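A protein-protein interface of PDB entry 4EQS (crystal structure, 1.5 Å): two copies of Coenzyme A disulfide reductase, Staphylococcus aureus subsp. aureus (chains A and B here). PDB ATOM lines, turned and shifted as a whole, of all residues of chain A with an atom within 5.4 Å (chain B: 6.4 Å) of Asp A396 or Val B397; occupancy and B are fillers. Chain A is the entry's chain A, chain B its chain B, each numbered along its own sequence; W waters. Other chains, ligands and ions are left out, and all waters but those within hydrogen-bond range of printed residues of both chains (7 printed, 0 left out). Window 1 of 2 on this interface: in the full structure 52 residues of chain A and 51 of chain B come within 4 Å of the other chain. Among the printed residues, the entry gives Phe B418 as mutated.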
ATOM      1  N   ASN A 322     -29.164  29.358 -17.707  1.00  0.00           N
ATOM      2  CA  ASN A 322     -29.004  28.124 -18.465  1.00  0.00           C
ATOM      3  C   ASN A 322     -28.314  27.082 -17.598  1.00  0.00           C
ATOM      4  O   ASN A 322     -27.293  27.365 -16.971  1.00  0.00           O
ATOM      5  CB  ASN A 322     -28.201  28.375 -19.743  1.00  0.00           C
ATOM      6  CG  ASN A 322     -28.474  27.336 -20.811  1.00  0.00           C
ATOM      7  OD1 ASN A 322     -29.106  26.311 -20.545  1.00  0.00           O
ATOM      8  ND2 ASN A 322     -27.992  27.589 -22.026  1.00  0.00           N
ATOM      9  N   ALA A 391     -31.039  17.454 -26.356  1.00  0.00           N
ATOM     10  CA  ALA A 391     -31.584  18.425 -25.413  1.00  0.00           C
ATOM     11  C   ALA A 391     -30.649  19.612 -25.197  1.00  0.00           C
ATOM     12  O   ALA A 391     -31.099  20.764 -25.147  1.00  0.00           O
ATOM     13  CB  ALA A 391     -31.912  17.754 -24.078  1.00  0.00           C
ATOM     14  N   ASP A 392     -29.350  19.348 -25.064  1.00  0.00           N
ATOM     15  CA  ASP A 392     -28.405  20.446 -24.906  1.00  0.00           C
ATOM     16  C   ASP A 392     -28.411  21.372 -26.126  1.00  0.00           C
ATOM     17  O   ASP A 392     -28.343  22.591 -25.985  1.00  0.00           O
ATOM     18  CB  ASP A 392     -26.981  19.964 -24.568  1.00  0.00           C
ATOM     19  CG  ASP A 392     -26.485  18.868 -25.491  1.00  0.00           C
ATOM     20  OD1 ASP A 392     -25.298  18.928 -25.891  1.00  0.00           O
ATOM     21  OD2 ASP A 392     -27.268  17.953 -25.811  1.00  0.00           O
ATOM     22  N   LYS A 393     -28.503  20.795 -27.320  1.00  0.00           N
ATOM     23  CA  LYS A 393     -28.525  21.605 -28.539  1.00  0.00           C
ATOM     24  C   LYS A 393     -29.738  22.542 -28.588  1.00  0.00           C
ATOM     25  O   LYS A 393     -29.596  23.725 -28.885  1.00  0.00           O
ATOM     26  CB  LYS A 393     -28.470  20.720 -29.790  1.00  0.00           C
ATOM     27  CG  LYS A 393     -28.560  21.511 -31.102  1.00  0.00           C
ATOM     28  CD  LYS A 393     -28.139  20.687 -32.324  1.00  0.00           C
ATOM     29  CE  LYS A 393     -29.105  19.542 -32.584  1.00  0.00           C
ATOM     30  NZ  LYS A 393     -28.722  18.778 -33.818  1.00  0.00           N
ATOM     31  N   ARG A 394     -30.916  22.032 -28.257  1.00  0.00           N
ATOM     32  CA  ARG A 394     -32.119  22.857 -28.361  1.00  0.00           C
ATOM     33  C   ARG A 394     -32.088  23.969 -27.310  1.00  0.00           C
ATOM     34  O   ARG A 394     -32.470  25.105 -27.586  1.00  0.00           O
ATOM     35  CB  ARG A 394     -33.405  22.031 -28.198  1.00  0.00           C
ATOM     36  CG  ARG A 394     -33.605  20.886 -29.210  1.00  0.00           C
ATOM     37  CD  ARG A 394     -33.057  21.243 -30.579  1.00  0.00           C
ATOM     38  NE  ARG A 394     -33.484  20.344 -31.660  1.00  0.00           N
ATOM     39  CZ  ARG A 394     -32.991  19.125 -31.885  1.00  0.00           C
ATOM     40  NH1 ARG A 394     -33.425  18.412 -32.926  1.00  0.00           N
ATOM     41  NH2 ARG A 394     -32.082  18.600 -31.078  1.00  0.00           N
ATOM     42  N   ILE A 395     -31.648  23.638 -26.105  1.00  0.00           N
ATOM     43  CA  ILE A 395     -31.654  24.621 -25.029  1.00  0.00           C
ATOM     44  C   ILE A 395     -30.592  25.701 -25.250  1.00  0.00           C
ATOM     45  O   ILE A 395     -30.828  26.867 -24.954  1.00  0.00           O
ATOM     46  CB  ILE A 395     -31.542  23.955 -23.638  1.00  0.00           C
ATOM     47  CG1 ILE A 395     -32.837  23.198 -23.326  1.00  0.00           C
ATOM     48  CG2 ILE A 395     -31.305  24.999 -22.561  1.00  0.00           C
ATOM     49  CD1 ILE A 395     -34.108  24.029 -23.518  1.00  0.00           C
ATOM     50  N   ASP A 396     -29.448  25.337 -25.817  1.00  0.00           N
ATOM     51  CA  ASP A 396     -28.457  26.357 -26.163  1.00  0.00           C
ATOM     52  C   ASP A 396     -28.971  27.300 -27.252  1.00  0.00           C
ATOM     53  O   ASP A 396     -28.741  28.510 -27.195  1.00  0.00           O
ATOM     54  CB  ASP A 396     -27.133  25.725 -26.590  1.00  0.00           C
ATOM     55  CG  ASP A 396     -26.199  25.470 -25.416  1.00  0.00           C
ATOM     56  OD1 ASP A 396     -26.523  25.872 -24.261  1.00  0.00           O
ATOM     57  OD2 ASP A 396     -25.122  24.880 -25.656  1.00  0.00           O
ATOM     58  N   VAL A 397     -29.667  26.752 -28.249  1.00  0.00           N
ATOM     59  CA  VAL A 397     -30.246  27.608 -29.273  1.00  0.00           C
ATOM     60  C   VAL A 397     -31.254  28.578 -28.648  1.00  0.00           C
ATOM     61  O   VAL A 397     -31.298  29.758 -28.997  1.00  0.00           O
ATOM     62  CB  VAL A 397     -30.916  26.788 -30.401  1.00  0.00           C
ATOM     63  CG1 VAL A 397     -31.781  27.689 -31.283  1.00  0.00           C
ATOM     64  CG2 VAL A 397     -29.867  26.075 -31.230  1.00  0.00           C
ATOM     65  N   LEU A 398     -32.061  28.085 -27.716  1.00  0.00           N
ATOM     66  CA  LEU A 398     -33.092  28.926 -27.124  1.00  0.00           C
ATOM     67  C   LEU A 398     -32.486  29.962 -26.171  1.00  0.00           C
ATOM     68  O   LEU A 398     -33.013  31.063 -26.040  1.00  0.00           O
ATOM     69  CB  LEU A 398     -34.180  28.079 -26.453  1.00  0.00           C
ATOM     70  CG  LEU A 398     -35.022  27.303 -27.478  1.00  0.00           C
ATOM     71  CD1 LEU A 398     -35.982  26.354 -26.773  1.00  0.00           C
ATOM     72  CD2 LEU A 398     -35.786  28.253 -28.396  1.00  0.00           C
ATOM     73  N   SER A 399     -31.364  29.622 -25.538  1.00  0.00           N
ATOM     74  CA  SER A 399     -30.630  30.600 -24.736  1.00  0.00           C
ATOM     75  C   SER A 399     -30.213  31.772 -25.624  1.00  0.00           C
ATOM     76  O   SER A 399     -30.368  32.940 -25.258  1.00  0.00           O
ATOM     77  CB  SER A 399     -29.396  29.961 -24.103  1.00  0.00           C
ATOM     78  OG  SER A 399     -28.657  30.938 -23.390  1.00  0.00           O
ATOM     79  N   MET A 400     -29.686  31.450 -26.804  1.00  0.00           N
ATOM     80  CA  MET A 400     -29.259  32.474 -27.741  1.00  0.00           C
ATOM     81  C   MET A 400     -30.468  33.289 -28.192  1.00  0.00           C
ATOM     82  O   MET A 400     -30.374  34.501 -28.385  1.00  0.00           O
ATOM     83  CB  MET A 400     -28.542  31.847 -28.941  1.00  0.00           C
ATOM     84  CG  MET A 400     -28.150  32.838 -30.035  1.00  0.00           C
ATOM     85  SD  MET A 400     -27.029  34.149 -29.494  1.00  0.00           S
ATOM     86  CE  MET A 400     -25.512  33.229 -29.285  1.00  0.00           C
ATOM     87  N   ALA A 401     -31.610  32.624 -28.350  1.00  0.00           N
ATOM     88  CA  ALA A 401     -32.827  33.326 -28.750  1.00  0.00           C
ATOM     89  C   ALA A 401     -33.272  34.303 -27.663  1.00  0.00           C
ATOM     90  O   ALA A 401     -33.606  35.455 -27.940  1.00  0.00           O
ATOM     91  CB  ALA A 401     -33.934  32.330 -29.074  1.00  0.00           C
ATOM     92  N   ASP B 392     -22.720  20.364 -34.659  1.00  0.00           N
ATOM     93  CA  ASP B 392     -24.100  20.735 -34.960  1.00  0.00           C
ATOM     94  C   ASP B 392     -24.643  21.723 -33.927  1.00  0.00           C
ATOM     95  O   ASP B 392     -25.358  22.668 -34.262  1.00  0.00           O
ATOM     96  CB  ASP B 392     -25.020  19.507 -35.115  1.00  0.00           C
ATOM     97  CG  ASP B 392     -24.973  18.566 -33.925  1.00  0.00           C
ATOM     98  OD1 ASP B 392     -26.015  17.943 -33.628  1.00  0.00           O
ATOM     99  OD2 ASP B 392     -23.909  18.437 -33.288  1.00  0.00           O
ATOM    100  N   LYS B 393     -24.271  21.520 -32.670  1.00  0.00           N
ATOM    101  CA  LYS B 393     -24.748  22.399 -31.615  1.00  0.00           C
ATOM    102  C   LYS B 393     -24.191  23.805 -31.809  1.00  0.00           C
ATOM    103  O   LYS B 393     -24.937  24.787 -31.755  1.00  0.00           O
ATOM    104  CB  LYS B 393     -24.378  21.847 -30.242  1.00  0.00           C
ATOM    105  CG  LYS B 393     -24.789  22.775 -29.095  1.00  0.00           C
ATOM    106  CD  LYS B 393     -24.813  22.057 -27.751  1.00  0.00           C
ATOM    107  CE  LYS B 393     -23.406  21.709 -27.281  1.00  0.00           C
ATOM    108  NZ  LYS B 393     -23.435  21.044 -25.935  1.00  0.00           N
ATOM    109  N   ARG B 394     -22.887  23.915 -32.053  1.00  0.00           N
ATOM    110  CA  ARG B 394     -22.291  25.241 -32.199  1.00  0.00           C
ATOM    111  C   ARG B 394     -22.862  25.974 -33.415  1.00  0.00           C
ATOM    112  O   ARG B 394     -23.164  27.161 -33.346  1.00  0.00           O
ATOM    113  CB  ARG B 394     -20.757  25.192 -32.278  1.00  0.00           C
ATOM    114  CG  ARG B 394     -20.048  24.541 -31.085  1.00  0.00           C
ATOM    115  CD  ARG B 394     -20.830  24.729 -29.808  1.00  0.00           C
ATOM    116  NE  ARG B 394     -20.075  24.401 -28.591  1.00  0.00           N
ATOM    117  CZ  ARG B 394     -19.886  23.169 -28.124  1.00  0.00           C
ATOM    118  NH1 ARG B 394     -19.228  22.988 -26.990  1.00  0.00           N
ATOM    119  NH2 ARG B 394     -20.347  22.116 -28.779  1.00  0.00           N
ATOM    120  N   ILE B 395     -23.027  25.268 -34.530  1.00  0.00           N
ATOM    121  CA  ILE B 395     -23.517  25.927 -35.741  1.00  0.00           C
ATOM    122  C   ILE B 395     -24.995  26.344 -35.645  1.00  0.00           C
ATOM    123  O   ILE B 395     -25.366  27.426 -36.111  1.00  0.00           O
ATOM    124  CB  ILE B 395     -23.229  25.091 -37.007  1.00  0.00           C
ATOM    125  CG1 ILE B 395     -21.715  24.957 -37.189  1.00  0.00           C
ATOM    126  CG2 ILE B 395     -23.849  25.758 -38.234  1.00  0.00           C
ATOM    127  CD1 ILE B 395     -20.992  26.300 -37.254  1.00  0.00           C
ATOM    128  N   ASP B 396     -25.827  25.523 -35.010  1.00  0.00           N
ATOM    129  CA  ASP B 396     -27.215  25.933 -34.771  1.00  0.00           C
ATOM    130  C   ASP B 396     -27.290  27.169 -33.869  1.00  0.00           C
ATOM    131  O   ASP B 396     -28.103  28.057 -34.099  1.00  0.00           O
ATOM    132  CB  ASP B 396     -28.041  24.791 -34.176  1.00  0.00           C
ATOM    133  CG  ASP B 396     -28.573  23.832 -35.233  1.00  0.00           C
ATOM    134  OD1 ASP B 396     -28.425  24.098 -36.450  1.00  0.00           O
ATOM    135  OD2 ASP B 396     -29.156  22.805 -34.841  1.00  0.00           O
ATOM    136  N   VAL B 397     -26.443  27.233 -32.840  1.00  0.00           N
ATOM    137  CA  VAL B 397     -26.430  28.407 -31.977  1.00  0.00           C
ATOM    138  C   VAL B 397     -26.016  29.639 -32.771  1.00  0.00           C
ATOM    139  O   VAL B 397     -26.621  30.707 -32.653  1.00  0.00           O
ATOM    140  CB  VAL B 397     -25.500  28.220 -30.754  1.00  0.00           C
ATOM    141  CG1 VAL B 397     -25.270  29.550 -30.038  1.00  0.00           C
ATOM    142  CG2 VAL B 397     -26.084  27.181 -29.811  1.00  0.00           C
ATOM    143  N   LEU B 398     -25.005  29.482 -33.616  1.00  0.00           N
ATOM    144  CA  LEU B 398     -24.551  30.609 -34.413  1.00  0.00           C
ATOM    145  C   LEU B 398     -25.566  31.003 -35.489  1.00  0.00           C
ATOM    146  O   LEU B 398     -25.665  32.175 -35.832  1.00  0.00           O
ATOM    147  CB  LEU B 398     -23.169  30.339 -35.000  1.00  0.00           C
ATOM    148  CG  LEU B 398     -22.074  30.298 -33.932  1.00  0.00           C
ATOM    149  CD1 LEU B 398     -20.785  29.765 -34.527  1.00  0.00           C
ATOM    150  CD2 LEU B 398     -21.848  31.662 -33.285  1.00  0.00           C
ATOM    151  N   SER B 399     -26.325  30.038 -36.002  1.00  0.00           N
ATOM    152  CA  SER B 399     -27.419  30.357 -36.922  1.00  0.00           C
ATOM    153  C   SER B 399     -28.424  31.284 -36.229  1.00  0.00           C
ATOM    154  O   SER B 399     -28.868  32.287 -36.793  1.00  0.00           O
ATOM    155  CB  SER B 399     -28.108  29.082 -37.410  1.00  0.00           C
ATOM    156  OG  SER B 399     -29.221  29.395 -38.238  1.00  0.00           O
ATOM    157  N   MET B 400     -28.769  30.953 -34.988  1.00  0.00           N
ATOM    158  CA  MET B 400     -29.684  31.786 -34.209  1.00  0.00           C
ATOM    159  C   MET B 400     -29.085  33.166 -33.911  1.00  0.00           C
ATOM    160  O   MET B 400     -29.788  34.179 -33.924  1.00  0.00           O
ATOM    161  CB  MET B 400     -30.070  31.067 -32.916  1.00  0.00           C
ATOM    162  CG  MET B 400     -30.967  31.892 -31.998  1.00  0.00           C
ATOM    163  SD  MET B 400     -32.587  32.295 -32.696  1.00  0.00           S
ATOM    164  CE  MET B 400     -33.396  30.714 -32.592  1.00  0.00           C
ATOM    165  N   ALA B 401     -27.784  33.207 -33.657  1.00  0.00           N
ATOM    166  CA  ALA B 401     -27.104  34.479 -33.448  1.00  0.00           C
ATOM    167  C   ALA B 401     -27.189  35.370 -34.681  1.00  0.00           C
ATOM    168  O   ALA B 401     -27.456  36.568 -34.579  1.00  0.00           O
ATOM    169  CB  ALA B 401     -25.648  34.238 -33.078  1.00  0.00           C
ATOM    170  N   MET B 402     -26.961  34.783 -35.852  1.00  0.00           N
ATOM    171  CA  MET B 402     -26.966  35.561 -37.083  1.00  0.00           C
ATOM    172  C   MET B 402     -28.373  36.057 -37.426  1.00  0.00           C
ATOM    173  O   MET B 402     -28.536  37.133 -37.990  1.00  0.00           O
ATOM    174  CB  MET B 402     -26.364  34.743 -38.221  1.00  0.00           C
ATOM    175  CG  MET B 402     -24.916  34.388 -37.952  1.00  0.00           C
ATOM    176  SD  MET B 402     -24.300  33.028 -38.951  1.00  0.00           S
ATOM    177  CE  MET B 402     -24.033  33.882 -40.489  1.00  0.00           C
ATOM    178  N   LEU B 411     -20.666  37.454 -28.649  1.00  0.00           N
ATOM    179  CA  LEU B 411     -20.589  36.023 -28.389  1.00  0.00           C
ATOM    180  C   LEU B 411     -20.027  35.714 -27.001  1.00  0.00           C
ATOM    181  O   LEU B 411     -20.252  34.626 -26.470  1.00  0.00           O
ATOM    182  CB  LEU B 411     -19.781  35.303 -29.467  1.00  0.00           C
ATOM    183  CG  LEU B 411     -20.425  35.299 -30.854  1.00  0.00           C
ATOM    184  CD1 LEU B 411     -19.500  34.649 -31.867  1.00  0.00           C
ATOM    185  CD2 LEU B 411     -21.785  34.598 -30.827  1.00  0.00           C
ATOM    186  N   PHE B 414     -22.985  34.911 -24.700  1.00  0.00           N
ATOM    187  CA  PHE B 414     -23.796  33.712 -24.868  1.00  0.00           C
ATOM    188  C   PHE B 414     -23.702  32.838 -23.624  1.00  0.00           C
ATOM    189  O   PHE B 414     -22.620  32.412 -23.229  1.00  0.00           O
ATOM    190  CB  PHE B 414     -23.366  32.940 -26.123  1.00  0.00           C
ATOM    191  CG  PHE B 414     -23.824  31.499 -26.153  1.00  0.00           C
ATOM    192  CD1 PHE B 414     -25.173  31.175 -26.180  1.00  0.00           C
ATOM    193  CD2 PHE B 414     -22.897  30.470 -26.176  1.00  0.00           C
ATOM    194  CE1 PHE B 414     -25.585  29.842 -26.215  1.00  0.00           C
ATOM    195  CE2 PHE B 414     -23.303  29.134 -26.206  1.00  0.00           C
ATOM    196  CZ  PHE B 414     -24.649  28.826 -26.234  1.00  0.00           C
ATOM    197  N   GLU B 415     -24.844  32.565 -23.010  1.00  0.00           N
ATOM    198  CA  GLU B 415     -24.855  31.770 -21.783  1.00  0.00           C
ATOM    199  C   GLU B 415     -25.104  30.297 -22.106  1.00  0.00           C
ATOM    200  O   GLU B 415     -26.236  29.864 -22.352  1.00  0.00           O
ATOM    201  CB  GLU B 415     -25.886  32.320 -20.795  1.00  0.00           C
ATOM    202  CG  GLU B 415     -25.849  31.632 -19.439  1.00  0.00           C
ATOM    203  CD  GLU B 415     -26.768  32.290 -18.430  1.00  0.00           C
ATOM    204  OE1 GLU B 415     -27.265  31.577 -17.532  1.00  0.00           O
ATOM    205  OE2 GLU B 415     -26.982  33.516 -18.536  1.00  0.00           O
ATOM    206  N   VAL B 416     -24.022  29.530 -22.127  1.00  0.00           N
ATOM    207  CA  VAL B 416     -24.087  28.134 -22.525  1.00  0.00           C
ATOM    208  C   VAL B 416     -24.626  27.262 -21.397  1.00  0.00           C
ATOM    209  O   VAL B 416     -24.547  27.626 -20.219  1.00  0.00           O
ATOM    210  CB  VAL B 416     -22.684  27.628 -22.940  1.00  0.00           C
ATOM    211  CG1 VAL B 416     -21.792  27.476 -21.711  1.00  0.00           C
ATOM    212  CG2 VAL B 416     -22.777  26.304 -23.698  1.00  0.00           C
ATOM    213  N   ALA B 417     -25.173  26.110 -21.764  1.00  0.00           N
ATOM    214  CA  ALA B 417     -25.536  25.104 -20.777  1.00  0.00           C
ATOM    215  C   ALA B 417     -24.290  24.296 -20.459  1.00  0.00           C
ATOM    216  O   ALA B 417     -23.828  23.507 -21.283  1.00  0.00           O
ATOM    217  CB  ALA B 417     -26.629  24.204 -21.324  1.00  0.00           C
ATOM    218  N   PHE B 418     -23.723  24.509 -19.273  1.00  0.00           N
ATOM    219  CA  PHE B 418     -22.507  23.788 -18.919  1.00  0.00           C
ATOM    220  C   PHE B 418     -22.642  22.755 -17.812  1.00  0.00           C
ATOM    221  O   PHE B 418     -23.061  23.056 -16.692  1.00  0.00           O
ATOM    222  CB  PHE B 418     -21.357  24.716 -18.536  1.00  0.00           C
ATOM    223  CG  PHE B 418     -20.198  23.974 -17.940  1.00  0.00           C
ATOM    224  CD1 PHE B 418     -19.386  23.196 -18.745  1.00  0.00           C
ATOM    225  CD2 PHE B 418     -19.956  24.002 -16.575  1.00  0.00           C
ATOM    226  CE1 PHE B 418     -18.327  22.481 -18.213  1.00  0.00           C
ATOM    227  CE2 PHE B 418     -18.896  23.291 -16.030  1.00  0.00           C
ATOM    228  CZ  PHE B 418     -18.080  22.528 -16.850  1.00  0.00           C
ATOM    229  N   TYR B 422     -20.946  18.278 -21.690  1.00  0.00           N
ATOM    230  CA  TYR B 422     -21.556  19.075 -22.756  1.00  0.00           C
ATOM    231  C   TYR B 422     -20.761  20.234 -23.351  1.00  0.00           C
ATOM    232  O   TYR B 422     -20.931  20.551 -24.530  1.00  0.00           O
ATOM    233  CB  TYR B 422     -22.921  19.601 -22.297  1.00  0.00           C
ATOM    234  CG  TYR B 422     -23.816  18.500 -21.796  1.00  0.00           C
ATOM    235  CD1 TYR B 422     -23.968  18.269 -20.433  1.00  0.00           C
ATOM    236  CD2 TYR B 422     -24.483  17.667 -22.689  1.00  0.00           C
ATOM    237  CE1 TYR B 422     -24.784  17.255 -19.972  1.00  0.00           C
ATOM    238  CE2 TYR B 422     -25.295  16.648 -22.237  1.00  0.00           C
ATOM    239  CZ  TYR B 422     -25.436  16.445 -20.880  1.00  0.00           C
ATOM    240  OH  TYR B 422     -26.242  15.425 -20.439  1.00  0.00           O
ATOM    241  N   SER B 423     -19.932  20.890 -22.549  1.00  0.00           N
ATOM    242  CA  SER B 423     -19.294  22.126 -22.987  1.00  0.00           C
ATOM    243  C   SER B 423     -18.211  22.547 -21.998  1.00  0.00           C
ATOM    244  O   SER B 423     -17.626  21.702 -21.328  1.00  0.00           O
ATOM    245  CB  SER B 423     -20.347  23.234 -23.096  1.00  0.00           C
ATOM    246  OG  SER B 423     -20.959  23.452 -21.829  1.00  0.00           O
ATOM    247  N   ASP B 427     -17.562  28.547 -23.280  1.00  0.00           N
ATOM    248  CA  ASP B 427     -17.722  27.655 -24.417  1.00  0.00           C
ATOM    249  C   ASP B 427     -16.856  28.098 -25.584  1.00  0.00           C
ATOM    250  O   ASP B 427     -16.386  29.238 -25.622  1.00  0.00           O
ATOM    251  CB  ASP B 427     -19.180  27.601 -24.870  1.00  0.00           C
ATOM    252  CG  ASP B 427     -19.406  26.527 -25.904  1.00  0.00           C
ATOM    253  OD1 ASP B 427     -19.913  26.836 -27.009  1.00  0.00           O
ATOM    254  OD2 ASP B 427     -19.022  25.375 -25.613  1.00  0.00           O
ATOM    255  N   ILE B 429     -17.926  28.954 -28.325  1.00  0.00           N
ATOM    256  CA  ILE B 429     -18.583  30.141 -28.840  1.00  0.00           C
ATOM    257  C   ILE B 429     -18.155  31.396 -28.072  1.00  0.00           C
ATOM    258  O   ILE B 429     -17.905  32.441 -28.674  1.00  0.00           O
ATOM    259  CB  ILE B 429     -20.120  29.984 -28.858  1.00  0.00           C
ATOM    260  CG1 ILE B 429     -20.515  28.967 -29.934  1.00  0.00           C
ATOM    261  CG2 ILE B 429     -20.804  31.323 -29.121  1.00  0.00           C
ATOM    262  CD1 ILE B 429     -21.986  28.605 -29.928  1.00  0.00           C
HETATM  263  O   HOH W   1     -31.343  22.414 -33.247  1.00  0.00           O
HETATM  264  O   HOH W   2     -24.254  22.890 -24.023  1.00  0.00           O
HETATM  265  O   HOH W   3     -25.581  29.868 -16.170  1.00  0.00           O
HETATM  266  O   HOH W   4     -24.750  26.718 -17.711  1.00  0.00           O
HETATM  267  O   HOH W   5     -28.798  20.505 -36.031  1.00  0.00           O
HETATM  268  O   HOH W   6     -27.274  33.301 -24.215  1.00  0.00           O
HETATM  269  O   HOH W   7     -22.881  25.231 -27.290  1.00  0.00           O
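The side-chain amide nitrogen of Asn A322 is in hydrogen-bond range of the backbone carbonyl oxygen of Glu B415 (2.9 Å). The backbone NH (N) of Ala B417 sits close to the side-chain amide nitrogen (ND2) of Asn A322. The side-chain carboxylate (OD1) of Asp A392 is in salt-bridge range of the side-chain amino group (NZ) of Lys B393 (2.8 Å). The side-chain carboxylate (OD1) of Asp B392 lies within salt-bridge range of the side-chain amino group (NZ) of Lys A393 (2.8 Å). The backbone NH (N) of Ala B417 is in hydrogen-bond range of the side-chain carboxylate (OD1) of Asp A396 (2.8 Å). OG of Ser A399 lies within hydrogen-bond range of O of Glu B415 (2.8 Å).
ND2 of Asn A322 lies within hydrogen-bond range of OD1 of Asp A396 (3.2 Å). The side-chain amino group of Lys B393 sits at hydrogen-bond distance from the backbone carbonyl oxygen of Tyr B422. OG of Ser B423 lies within hydrogen-bond range of O of Ala B417 (2.9 Å).
ND2 of Asn A322 touches C of Val B416, at 3.4 Å. Tyr B422 touches Asp A392. Asp B396 touches Lys A393. Val B397 touches Asp A396. Asp A396 touches Phe B414 (O to CE1, 3.6 Å). Asp A396 touches Val B416 (OD2 to CG2, 3.4 Å). CG2 of Val A397 touches CB of Asp B396, at 3.7 Å. CG1 of Val A397 touches CE of Met B400, at 3.7 Å. Val B397 touches Met A400. Ala A401 touches Met B400 (N to CG, 3.8 Å).
Val B397 touches just these residues of chain A: Asp A396, Val A397 and Met A400. Of the printed residues of chain B, Asn A322 touches Glu B415 (2.9 Å), Val B416 (3.4 Å) and Ala B417 (3.2 Å). Printed residues of chain A within 4 Å of Val B416: Asn A322 (3.4 Å) and Asp A396 (3.4 Å). Ala A391 touches none of the printed residues of chain B. Arg B394 touches none of the printed residues of chain A. The nearest residue of chain B that does not touch Asp A396 is Glu B415 (4.4 Å). The nearest residue of chain A that does not touch Val B397 is Lys A393 (5.0 Å).
Of the 21 printed residues of chain B, 11 touch a printed residue of chain A. Hydrophobic or aromatic side chains of chain B within 4 Å of the printed part of chain A: Val B397, Met B400, Ala B401, Phe B414, Val B416, Ala B417 and Tyr B422. Of the 12 printed residues of chain A, 8 touch a printed residue of chain B. Hydrophobic or aromatic side chains of chain A within 4 Å of the printed part of chain B: Val A397, Met A400 and Ala A401. Among the printed residues, 22 pairs touch across the chains. Among the printed residues, Asp or Glu carboxylates within 4 Å of a Lys or Arg side-chain nitrogen of the other chain: Asp A392 with Lys B393 (2.8 Å) and Lys A393 with Asp B392 (2.8 Å).
Asp A396 touches Val B397, and with the chains exchanged Val A397 touches Asp B396. Val B397 touches its own counterpart, Val A397. Val A397 touches Met B400, and with the chains exchanged Met A400 touches Val B397. Met A400 touches Ala B401, and with the chains exchanged Ala A401 touches Met B400. 10 positions are printed for both chains.
Water W5 bridges the side-chain carboxylate (OD2) of Asp B396 and the side-chain amino group (NZ) of Lys A393. Water W4 lies within hydrogen-bond range of the backbone carbonyl oxygen (O) of Val B416, the backbone carbonyl oxygen (O) of Asn A322 and the backbone NH (N) of Phe B418. Water W2 lies within hydrogen-bond range of the side-chain carboxylate (OD2) of Asp A396 (2.7 Å), the side-chain amino group (NZ) of Lys B393 (2.8 Å) and the backbone carbonyl oxygen (O) of Ala B417 (2.8 Å). Water W3 bridges OE1 of Glu B415 (2.8 Å) and O of Asn A322 (3.1 Å). Water W7 lies within hydrogen-bond range of OD2 of Asp A396 (2.8 Å), NE of Arg B394 (3.2 Å) and OD1 of Asp B427 (3.4 Å). Water W6 lies within hydrogen-bond range of N of Glu B415 (2.8 Å) and OG of Ser A399 (2.9 Å).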
